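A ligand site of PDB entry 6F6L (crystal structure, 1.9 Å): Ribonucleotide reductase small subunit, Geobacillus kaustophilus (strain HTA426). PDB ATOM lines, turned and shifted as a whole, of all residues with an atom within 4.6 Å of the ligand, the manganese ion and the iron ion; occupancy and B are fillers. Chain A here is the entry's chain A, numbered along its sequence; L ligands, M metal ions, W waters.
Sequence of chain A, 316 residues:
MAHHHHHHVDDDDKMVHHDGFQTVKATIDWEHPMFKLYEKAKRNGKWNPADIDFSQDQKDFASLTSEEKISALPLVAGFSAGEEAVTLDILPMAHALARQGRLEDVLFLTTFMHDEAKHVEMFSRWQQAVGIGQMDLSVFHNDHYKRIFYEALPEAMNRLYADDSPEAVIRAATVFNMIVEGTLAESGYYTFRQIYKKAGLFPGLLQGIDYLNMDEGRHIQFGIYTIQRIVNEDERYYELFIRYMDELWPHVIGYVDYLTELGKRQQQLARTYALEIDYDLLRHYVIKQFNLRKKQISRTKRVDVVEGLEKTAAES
The backbone carbonyl oxygen (O) of Ser 187 sits at hydrogen-bond distance from the side-chain hydroxyl (OG1) of Thr 191 (2.8 Å).
The backbone carbonyl oxygen (O) of Val 180 is in hydrogen-bond range of the backbone NH (N) of Ala 185 (2.8 Å).
The backbone carbonyl oxygen (O) of Val 256 sits at hydrogen-bond distance from the side-chain hydroxyl (OG1) of Thr 260, at 3.0 Å.
Merely in contact with the ligand: Gly 78 (3.5 Å), Phe 79 (3.6 Å), Gly 82 (3.97 Å), Val 86 (3.8 Å), Phe 149 (3.7 Å), Val 180 (3.7 Å), Leu 184 (3.7 Å), Ala 185 (3.99 Å), Gly 188 (3.7 Å), Thr 191 (3.5 Å), Tyr 255 (3.9 Å), Val 256 (3.9 Å), Leu 259 (3.8 Å) and Thr 260 (3.98 Å).
The nearest printed residue that does not touch the ligand is Leu 282 (4.01 Å).
Four residues have an atom within 4 Å of the manganese ion: Glu 83, Glu 116, His 119 and Glu 216.
Of the 27 residues printed, 4 come within 4 Å of the iron ion.
The manganese ion is bound by an oxygen (O1) of the ligand, the side-chain carboxylate of Glu 116, the side-chain carboxylate of Glu 83, a ring nitrogen (ND1) of His 119, water W2 and water W1.
The manganese ion has six donor atoms within binding distance.
The iron ion is bound by OE2 of Glu 181, water W2, OE2 of Glu 116, O2 of the ligand, OE2 of Glu 216 and ND1 of His 219.
The iron ion has six donor atoms within binding distance.
Water W1 lies within hydrogen-bond range of OH of Tyr 189 (2.6 Å) and OE1 of Glu 216 (3.1 Å).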
ATOM      1  N   LEU A  75       2.380   2.923   8.286  1.00  0.00           N
ATOM      2  CA  LEU A  75       2.985   3.852   7.335  1.00  0.00           C
ATOM      3  C   LEU A  75       2.166   3.953   6.061  1.00  0.00           C
ATOM      4  O   LEU A  75       1.951   5.044   5.544  1.00  0.00           O
ATOM      5  CB  LEU A  75       4.405   3.404   7.010  1.00  0.00           C
ATOM      6  CG  LEU A  75       5.457   4.507   6.977  1.00  0.00           C
ATOM      7  CD1 LEU A  75       5.659   5.064   8.393  1.00  0.00           C
ATOM      8  CD2 LEU A  75       6.773   3.945   6.412  1.00  0.00           C
ATOM      9  N   GLY A  78      -0.967   5.955   6.549  1.00  0.00           N
ATOM     10  CA  GLY A  78      -0.782   7.394   6.594  1.00  0.00           C
ATOM     11  C   GLY A  78      -0.600   7.969   5.216  1.00  0.00           C
ATOM     12  O   GLY A  78      -1.128   9.040   4.889  1.00  0.00           O
ATOM     13  N   PHE A  79       0.182   7.279   4.387  1.00  0.00           N
ATOM     14  CA  PHE A  79       0.375   7.732   3.016  1.00  0.00           C
ATOM     15  C   PHE A  79      -0.908   7.650   2.215  1.00  0.00           C
ATOM     16  O   PHE A  79      -1.199   8.558   1.443  1.00  0.00           O
ATOM     17  CB  PHE A  79       1.446   6.927   2.321  1.00  0.00           C
ATOM     18  CG  PHE A  79       2.807   7.547   2.413  1.00  0.00           C
ATOM     19  CD1 PHE A  79       3.120   8.669   1.669  1.00  0.00           C
ATOM     20  CD2 PHE A  79       3.752   7.025   3.281  1.00  0.00           C
ATOM     21  CE1 PHE A  79       4.368   9.239   1.776  1.00  0.00           C
ATOM     22  CE2 PHE A  79       5.034   7.602   3.378  1.00  0.00           C
ATOM     23  CZ  PHE A  79       5.319   8.701   2.640  1.00  0.00           C
ATOM     24  N   GLY A  82      -3.112  10.396   3.091  1.00  0.00           N
ATOM     25  CA  GLY A  82      -2.422  11.620   2.737  1.00  0.00           C
ATOM     26  C   GLY A  82      -2.514  11.955   1.256  1.00  0.00           C
ATOM     27  O   GLY A  82      -2.840  13.091   0.888  1.00  0.00           O
ATOM     28  N   GLU A  83      -2.203  10.979   0.378  1.00  0.00           N
ATOM     29  CA  GLU A  83      -2.280  11.208  -1.069  1.00  0.00           C
ATOM     30  C   GLU A  83      -3.697  11.553  -1.478  1.00  0.00           C
ATOM     31  O   GLU A  83      -3.928  12.424  -2.334  1.00  0.00           O
ATOM     32  CB  GLU A  83      -1.819   9.959  -1.849  1.00  0.00           C
ATOM     33  CG  GLU A  83      -0.462   9.381  -1.473  1.00  0.00           C
ATOM     34  CD  GLU A  83       0.714  10.327  -1.688  1.00  0.00           C
ATOM     35  OE1 GLU A  83       0.534  11.370  -2.360  1.00  0.00           O
ATOM     36  OE2 GLU A  83       1.814  10.010  -1.174  1.00  0.00           O
ATOM     37  N   VAL A  86      -4.562  15.187  -0.329  1.00  0.00           N
ATOM     38  CA  VAL A  86      -3.948  16.262  -1.119  1.00  0.00           C
ATOM     39  C   VAL A  86      -4.476  16.259  -2.557  1.00  0.00           C
ATOM     40  O   VAL A  86      -4.533  17.319  -3.193  1.00  0.00           O
ATOM     41  CB  VAL A  86      -2.397  16.184  -1.095  1.00  0.00           C
ATOM     42  CG1 VAL A  86      -1.860  16.393   0.343  1.00  0.00           C
ATOM     43  CG2 VAL A  86      -1.899  14.888  -1.693  1.00  0.00           C
ATOM     44  N   PHE A 112       0.890  18.927 -10.756  1.00  0.00           N
ATOM     45  CA  PHE A 112       0.870  18.637  -9.324  1.00  0.00           C
ATOM     46  C   PHE A 112      -0.317  17.746  -8.987  1.00  0.00           C
ATOM     47  O   PHE A 112      -0.165  16.686  -8.358  1.00  0.00           O
ATOM     48  CB  PHE A 112       0.807  19.991  -8.589  1.00  0.00           C
ATOM     49  CG  PHE A 112       1.043  19.946  -7.113  1.00  0.00           C
ATOM     50  CD1 PHE A 112       1.552  21.059  -6.487  1.00  0.00           C
ATOM     51  CD2 PHE A 112       0.675  18.879  -6.331  1.00  0.00           C
ATOM     52  CE1 PHE A 112       1.783  21.063  -5.153  1.00  0.00           C
ATOM     53  CE2 PHE A 112       0.880  18.899  -4.966  1.00  0.00           C
ATOM     54  CZ  PHE A 112       1.417  19.972  -4.368  1.00  0.00           C
ATOM     55  N   GLU A 116      -0.471  13.677  -7.797  1.00  0.00           N
ATOM     56  CA  GLU A 116      -1.081  13.153  -6.594  1.00  0.00           C
ATOM     57  C   GLU A 116      -2.080  12.056  -6.935  1.00  0.00           C
ATOM     58  O   GLU A 116      -2.213  11.056  -6.190  1.00  0.00           O
ATOM     59  CB  GLU A 116      -1.741  14.252  -5.750  1.00  0.00           C
ATOM     60  CG  GLU A 116      -0.831  15.396  -5.324  1.00  0.00           C
ATOM     61  CD  GLU A 116       0.274  14.996  -4.370  1.00  0.00           C
ATOM     62  OE1 GLU A 116       0.444  13.779  -4.041  1.00  0.00           O
ATOM     63  OE2 GLU A 116       0.932  15.933  -3.884  1.00  0.00           O
ATOM     64  N   HIS A 119      -0.178   9.102  -7.170  1.00  0.00           N
ATOM     65  CA  HIS A 119       0.273   8.613  -5.874  1.00  0.00           C
ATOM     66  C   HIS A 119      -0.817   7.817  -5.155  1.00  0.00           C
ATOM     67  O   HIS A 119      -0.521   6.802  -4.511  1.00  0.00           O
ATOM     68  CB  HIS A 119       0.703   9.772  -5.001  1.00  0.00           C
ATOM     69  CG  HIS A 119       1.839  10.548  -5.589  1.00  0.00           C
ATOM     70  ND1 HIS A 119       2.426  11.612  -4.939  1.00  0.00           N
ATOM     71  CD2 HIS A 119       2.495  10.413  -6.760  1.00  0.00           C
ATOM     72  CE1 HIS A 119       3.405  12.093  -5.692  1.00  0.00           C
ATOM     73  NE2 HIS A 119       3.452  11.395  -6.823  1.00  0.00           N
ATOM     74  N   PHE A 149      -4.836  15.897   8.738  1.00  0.00           N
ATOM     75  CA  PHE A 149      -5.319  15.474   7.421  1.00  0.00           C
ATOM     76  C   PHE A 149      -6.836  15.470   7.284  1.00  0.00           C
ATOM     77  O   PHE A 149      -7.345  15.729   6.197  1.00  0.00           O
ATOM     78  CB  PHE A 149      -4.803  14.074   7.097  1.00  0.00           C
ATOM     79  CG  PHE A 149      -3.334  14.041   6.776  1.00  0.00           C
ATOM     80  CD1 PHE A 149      -2.883  14.322   5.508  1.00  0.00           C
ATOM     81  CD2 PHE A 149      -2.400  13.756   7.759  1.00  0.00           C
ATOM     82  CE1 PHE A 149      -1.546  14.303   5.194  1.00  0.00           C
ATOM     83  CE2 PHE A 149      -1.045  13.759   7.452  1.00  0.00           C
ATOM     84  CZ  PHE A 149      -0.635  14.014   6.160  1.00  0.00           C
ATOM     85  N   VAL A 180       2.693  18.888   5.457  1.00  0.00           N
ATOM     86  CA  VAL A 180       2.250  17.597   4.916  1.00  0.00           C
ATOM     87  C   VAL A 180       3.307  16.999   3.992  1.00  0.00           C
ATOM     88  O   VAL A 180       3.718  15.837   4.149  1.00  0.00           O
ATOM     89  CB  VAL A 180       0.892  17.755   4.240  1.00  0.00           C
ATOM     90  CG1 VAL A 180       0.538  16.511   3.352  1.00  0.00           C
ATOM     91  CG2 VAL A 180      -0.150  17.998   5.311  1.00  0.00           C
ATOM     92  N   GLU A 181       3.747  17.759   2.994  1.00  0.00           N
ATOM     93  CA  GLU A 181       4.692  17.266   1.999  1.00  0.00           C
ATOM     94  C   GLU A 181       6.147  17.392   2.475  1.00  0.00           C
ATOM     95  O   GLU A 181       6.881  16.398   2.509  1.00  0.00           O
ATOM     96  CB  GLU A 181       4.501  18.047   0.686  1.00  0.00           C
ATOM     97  CG  GLU A 181       3.238  17.625  -0.059  1.00  0.00           C
ATOM     98  CD  GLU A 181       2.988  18.417  -1.309  1.00  0.00           C
ATOM     99  OE1 GLU A 181       3.276  19.635  -1.265  1.00  0.00           O
ATOM    100  OE2 GLU A 181       2.530  17.818  -2.324  1.00  0.00           O
ATOM    101  N   LEU A 184       6.148  15.690   6.615  1.00  0.00           N
ATOM    102  CA  LEU A 184       5.694  14.325   6.872  1.00  0.00           C
ATOM    103  C   LEU A 184       5.987  13.390   5.696  1.00  0.00           C
ATOM    104  O   LEU A 184       6.555  12.315   5.901  1.00  0.00           O
ATOM    105  CB  LEU A 184       4.201  14.320   7.219  1.00  0.00           C
ATOM    106  CG  LEU A 184       3.874  14.846   8.607  1.00  0.00           C
ATOM    107  CD1 LEU A 184       2.372  15.094   8.664  1.00  0.00           C
ATOM    108  CD2 LEU A 184       4.311  13.866   9.680  1.00  0.00           C
ATOM    109  N   ALA A 185       5.663  13.787   4.460  1.00  0.00           N
ATOM    110  CA  ALA A 185       5.890  12.878   3.328  1.00  0.00           C
ATOM    111  C   ALA A 185       7.382  12.573   3.154  1.00  0.00           C
ATOM    112  O   ALA A 185       7.769  11.410   2.922  1.00  0.00           O
ATOM    113  CB  ALA A 185       5.335  13.464   2.033  1.00  0.00           C
ATOM    114  N   SER A 187       9.747  12.547   5.403  1.00  0.00           N
ATOM    115  CA  SER A 187      10.204  11.684   6.476  1.00  0.00           C
ATOM    116  C   SER A 187       9.660  10.280   6.309  1.00  0.00           C
ATOM    117  O   SER A 187      10.356   9.323   6.655  1.00  0.00           O
ATOM    118  CB  SER A 187       9.794  12.279   7.830  1.00  0.00           C
ATOM    119  OG  SER A 187      10.319  13.597   7.968  1.00  0.00           O
ATOM    120  N   GLY A 188       8.453  10.137   5.746  1.00  0.00           N
ATOM    121  CA  GLY A 188       7.940   8.826   5.370  1.00  0.00           C
ATOM    122  C   GLY A 188       8.752   8.134   4.280  1.00  0.00           C
ATOM    123  O   GLY A 188       8.960   6.908   4.340  1.00  0.00           O
ATOM    124  N   TYR A 189       9.162   8.869   3.244  1.00  0.00           N
ATOM    125  CA  TYR A 189      10.019   8.276   2.218  1.00  0.00           C
ATOM    126  C   TYR A 189      11.301   7.753   2.857  1.00  0.00           C
ATOM    127  O   TYR A 189      11.749   6.643   2.548  1.00  0.00           O
ATOM    128  CB  TYR A 189      10.407   9.285   1.138  1.00  0.00           C
ATOM    129  CG  TYR A 189       9.252   9.901   0.422  1.00  0.00           C
ATOM    130  CD1 TYR A 189       8.120   9.180   0.177  1.00  0.00           C
ATOM    131  CD2 TYR A 189       9.279  11.229   0.027  1.00  0.00           C
ATOM    132  CE1 TYR A 189       7.027   9.761  -0.461  1.00  0.00           C
ATOM    133  CE2 TYR A 189       8.196  11.808  -0.590  1.00  0.00           C
ATOM    134  CZ  TYR A 189       7.078  11.068  -0.838  1.00  0.00           C
ATOM    135  OH  TYR A 189       5.969  11.632  -1.453  1.00  0.00           O
ATOM    136  N   THR A 191      11.802   6.923   5.994  1.00  0.00           N
ATOM    137  CA  THR A 191      11.478   5.798   6.846  1.00  0.00           C
ATOM    138  C   THR A 191      11.321   4.511   6.037  1.00  0.00           C
ATOM    139  O   THR A 191      11.820   3.446   6.437  1.00  0.00           O
ATOM    140  CB  THR A 191      10.211   6.100   7.652  1.00  0.00           C
ATOM    141  OG1 THR A 191      10.430   7.231   8.501  1.00  0.00           O
ATOM    142  CG2 THR A 191       9.768   4.908   8.507  1.00  0.00           C
ATOM    143  N   GLU A 216       7.662  14.819  -5.445  1.00  0.00           N
ATOM    144  CA  GLU A 216       7.522  15.673  -4.254  1.00  0.00           C
ATOM    145  C   GLU A 216       8.421  16.884  -4.317  1.00  0.00           C
ATOM    146  O   GLU A 216       8.083  17.939  -3.779  1.00  0.00           O
ATOM    147  CB  GLU A 216       7.883  14.896  -2.999  1.00  0.00           C
ATOM    148  CG  GLU A 216       7.180  15.319  -1.747  1.00  0.00           C
ATOM    149  CD  GLU A 216       5.727  15.044  -1.908  1.00  0.00           C
ATOM    150  OE1 GLU A 216       5.341  13.904  -1.685  1.00  0.00           O
ATOM    151  OE2 GLU A 216       5.000  15.973  -2.338  1.00  0.00           O
ATOM    152  N   HIS A 219       6.625  19.591  -5.835  1.00  0.00           N
ATOM    153  CA  HIS A 219       5.516  20.045  -4.995  1.00  0.00           C
ATOM    154  C   HIS A 219       6.000  20.987  -3.908  1.00  0.00           C
ATOM    155  O   HIS A 219       5.381  22.033  -3.657  1.00  0.00           O
ATOM    156  CB  HIS A 219       4.792  18.838  -4.377  1.00  0.00           C
ATOM    157  CG  HIS A 219       4.251  17.882  -5.398  1.00  0.00           C
ATOM    158  ND1 HIS A 219       3.521  16.755  -5.090  1.00  0.00           N
ATOM    159  CD2 HIS A 219       4.371  17.883  -6.747  1.00  0.00           C
ATOM    160  CE1 HIS A 219       3.232  16.098  -6.201  1.00  0.00           C
ATOM    161  NE2 HIS A 219       3.728  16.776  -7.222  1.00  0.00           N
ATOM    162  N   TYR A 255       1.909  12.562  15.820  1.00  0.00           N
ATOM    163  CA  TYR A 255       1.728  11.418  14.913  1.00  0.00           C
ATOM    164  C   TYR A 255       2.992  10.581  14.882  1.00  0.00           C
ATOM    165  O   TYR A 255       2.923   9.349  15.035  1.00  0.00           O
ATOM    166  CB  TYR A 255       1.353  11.915  13.515  1.00  0.00           C
ATOM    167  CG  TYR A 255       1.224  10.834  12.481  1.00  0.00           C
ATOM    168  CD1 TYR A 255       0.357   9.773  12.663  1.00  0.00           C
ATOM    169  CD2 TYR A 255       1.931  10.905  11.313  1.00  0.00           C
ATOM    170  CE1 TYR A 255       0.213   8.799  11.712  1.00  0.00           C
ATOM    171  CE2 TYR A 255       1.819   9.903  10.336  1.00  0.00           C
ATOM    172  CZ  TYR A 255       0.950   8.864  10.553  1.00  0.00           C
ATOM    173  OH  TYR A 255       0.813   7.882   9.594  1.00  0.00           O
ATOM    174  N   VAL A 256       4.160  11.226  14.790  1.00  0.00           N
ATOM    175  CA  VAL A 256       5.422  10.507  14.671  1.00  0.00           C
ATOM    176  C   VAL A 256       5.684   9.658  15.915  1.00  0.00           C
ATOM    177  O   VAL A 256       6.075   8.503  15.817  1.00  0.00           O
ATOM    178  CB  VAL A 256       6.558  11.520  14.403  1.00  0.00           C
ATOM    179  CG1 VAL A 256       7.891  10.934  14.695  1.00  0.00           C
ATOM    180  CG2 VAL A 256       6.504  11.996  12.953  1.00  0.00           C
ATOM    181  N   LEU A 259       3.445   6.554  15.649  1.00  0.00           N
ATOM    182  CA  LEU A 259       4.050   5.539  14.791  1.00  0.00           C
ATOM    183  C   LEU A 259       5.247   4.891  15.458  1.00  0.00           C
ATOM    184  O   LEU A 259       5.459   3.681  15.311  1.00  0.00           O
ATOM    185  CB  LEU A 259       4.497   6.144  13.471  1.00  0.00           C
ATOM    186  CG  LEU A 259       3.379   6.598  12.536  1.00  0.00           C
ATOM    187  CD1 LEU A 259       4.019   7.268  11.328  1.00  0.00           C
ATOM    188  CD2 LEU A 259       2.516   5.434  12.124  1.00  0.00           C
ATOM    189  N   THR A 260       6.072   5.699  16.145  1.00  0.00           N
ATOM    190  CA  THR A 260       7.275   5.189  16.781  1.00  0.00           C
ATOM    191  C   THR A 260       6.924   4.196  17.868  1.00  0.00           C
ATOM    192  O   THR A 260       7.604   3.169  18.036  1.00  0.00           O
ATOM    193  CB  THR A 260       8.072   6.341  17.375  1.00  0.00           C
ATOM    194  OG1 THR A 260       8.644   7.118  16.318  1.00  0.00           O
ATOM    195  CG2 THR A 260       9.183   5.837  18.224  1.00  0.00           C
ATOM    196  N   TYR A 279      14.733   4.177  15.844  1.00  0.00           N
ATOM    197  CA  TYR A 279      13.571   5.064  15.873  1.00  0.00           C
ATOM    198  C   TYR A 279      13.945   6.463  16.333  1.00  0.00           C
ATOM    199  O   TYR A 279      13.227   7.417  16.027  1.00  0.00           O
ATOM    200  CB  TYR A 279      12.480   4.504  16.773  1.00  0.00           C
ATOM    201  CG  TYR A 279      11.757   3.383  16.113  1.00  0.00           C
ATOM    202  CD1 TYR A 279      10.900   3.617  15.050  1.00  0.00           C
ATOM    203  CD2 TYR A 279      11.966   2.063  16.515  1.00  0.00           C
ATOM    204  CE1 TYR A 279      10.259   2.577  14.409  1.00  0.00           C
ATOM    205  CE2 TYR A 279      11.323   1.020  15.887  1.00  0.00           C
ATOM    206  CZ  TYR A 279      10.473   1.272  14.837  1.00  0.00           C
ATOM    207  OH  TYR A 279       9.833   0.237  14.204  1.00  0.00           O
ATOM    208  N   LEU A 282      15.053   8.262  13.218  1.00  0.00           N
ATOM    209  CA  LEU A 282      13.880   8.647  12.437  1.00  0.00           C
ATOM    210  C   LEU A 282      13.255   9.912  12.996  1.00  0.00           C
ATOM    211  O   LEU A 282      13.003  10.870  12.247  1.00  0.00           O
ATOM    212  CB  LEU A 282      12.860   7.513  12.400  1.00  0.00           C
ATOM    213  CG  LEU A 282      13.410   6.249  11.704  1.00  0.00           C
ATOM    214  CD1 LEU A 282      12.452   5.050  11.772  1.00  0.00           C
ATOM    215  CD2 LEU A 282      13.793   6.520  10.245  1.00  0.00           C
ATOM    216  N   VAL A 286      12.607  13.819  11.221  1.00  0.00           N
ATOM    217  CA  VAL A 286      11.391  14.645  11.202  1.00  0.00           C
ATOM    218  C   VAL A 286      11.706  16.057  11.689  1.00  0.00           C
ATOM    219  O   VAL A 286      11.299  17.056  11.076  1.00  0.00           O
ATOM    220  CB  VAL A 286      10.290  13.995  12.050  1.00  0.00           C
ATOM    221  CG1 VAL A 286       9.078  14.922  12.195  1.00  0.00           C
ATOM    222  CG2 VAL A 286       9.875  12.696  11.415  1.00  0.00           C
HETATM  223  C1  LIG L   1       1.751  14.286  -0.797  1.00  0.00           C
HETATM  224  O1  LIG L   1       1.839  13.276  -1.519  1.00  0.00           O
HETATM  225  O2  LIG L   1       1.841  15.461  -1.167  1.00  0.00           O
HETATM  226  C2  LIG L   1       1.536  14.100   0.754  1.00  0.00           C
HETATM  227  C3  LIG L   1       1.484  12.696   1.348  1.00  0.00           C
HETATM  228  C4  LIG L   1       1.389  12.703   2.919  1.00  0.00           C
HETATM  229  C5  LIG L   1       1.934  11.430   3.622  1.00  0.00           C
HETATM  230  C6  LIG L   1       1.751  11.398   5.140  1.00  0.00           C
HETATM  231  C7  LIG L   1       2.130  10.045   5.840  1.00  0.00           C
HETATM  232  C8  LIG L   1       3.607   9.904   6.018  1.00  0.00           C
HETATM  233  C9  LIG L   1       4.073   9.095   7.223  1.00  0.00           C
HETATM  234  C10 LIG L   1       4.995   9.902   8.158  1.00  0.00           C
HETATM  235  C11 LIG L   1       6.190   9.162   8.598  1.00  0.00           C
HETATM  236  C12 LIG L   1       6.893   9.820   9.765  1.00  0.00           C
HETATM  237  C13 LIG L   1       8.022   8.950  10.314  1.00  0.00           C
HETATM  238  C14 LIG L   1       7.685   8.148  11.558  1.00  0.00           C
HETATM  239  C15 LIG L   1       8.864   7.297  12.086  1.00  0.00           C
HETATM  240  C16 LIG L   1       8.491   5.857  12.544  1.00  0.00           C
HETATM  241 MN    MN M   1       1.963  12.685  -3.144  1.00  0.00          MN
HETATM  242 FE    FE M   2       2.888  15.972  -3.054  1.00  0.00          FE
HETATM  243  O   HOH W   1       3.426  11.424  -1.875  1.00  0.00           O
HETATM  244  O   HOH W   2       3.555  14.100  -3.656  1.00  0.00           O
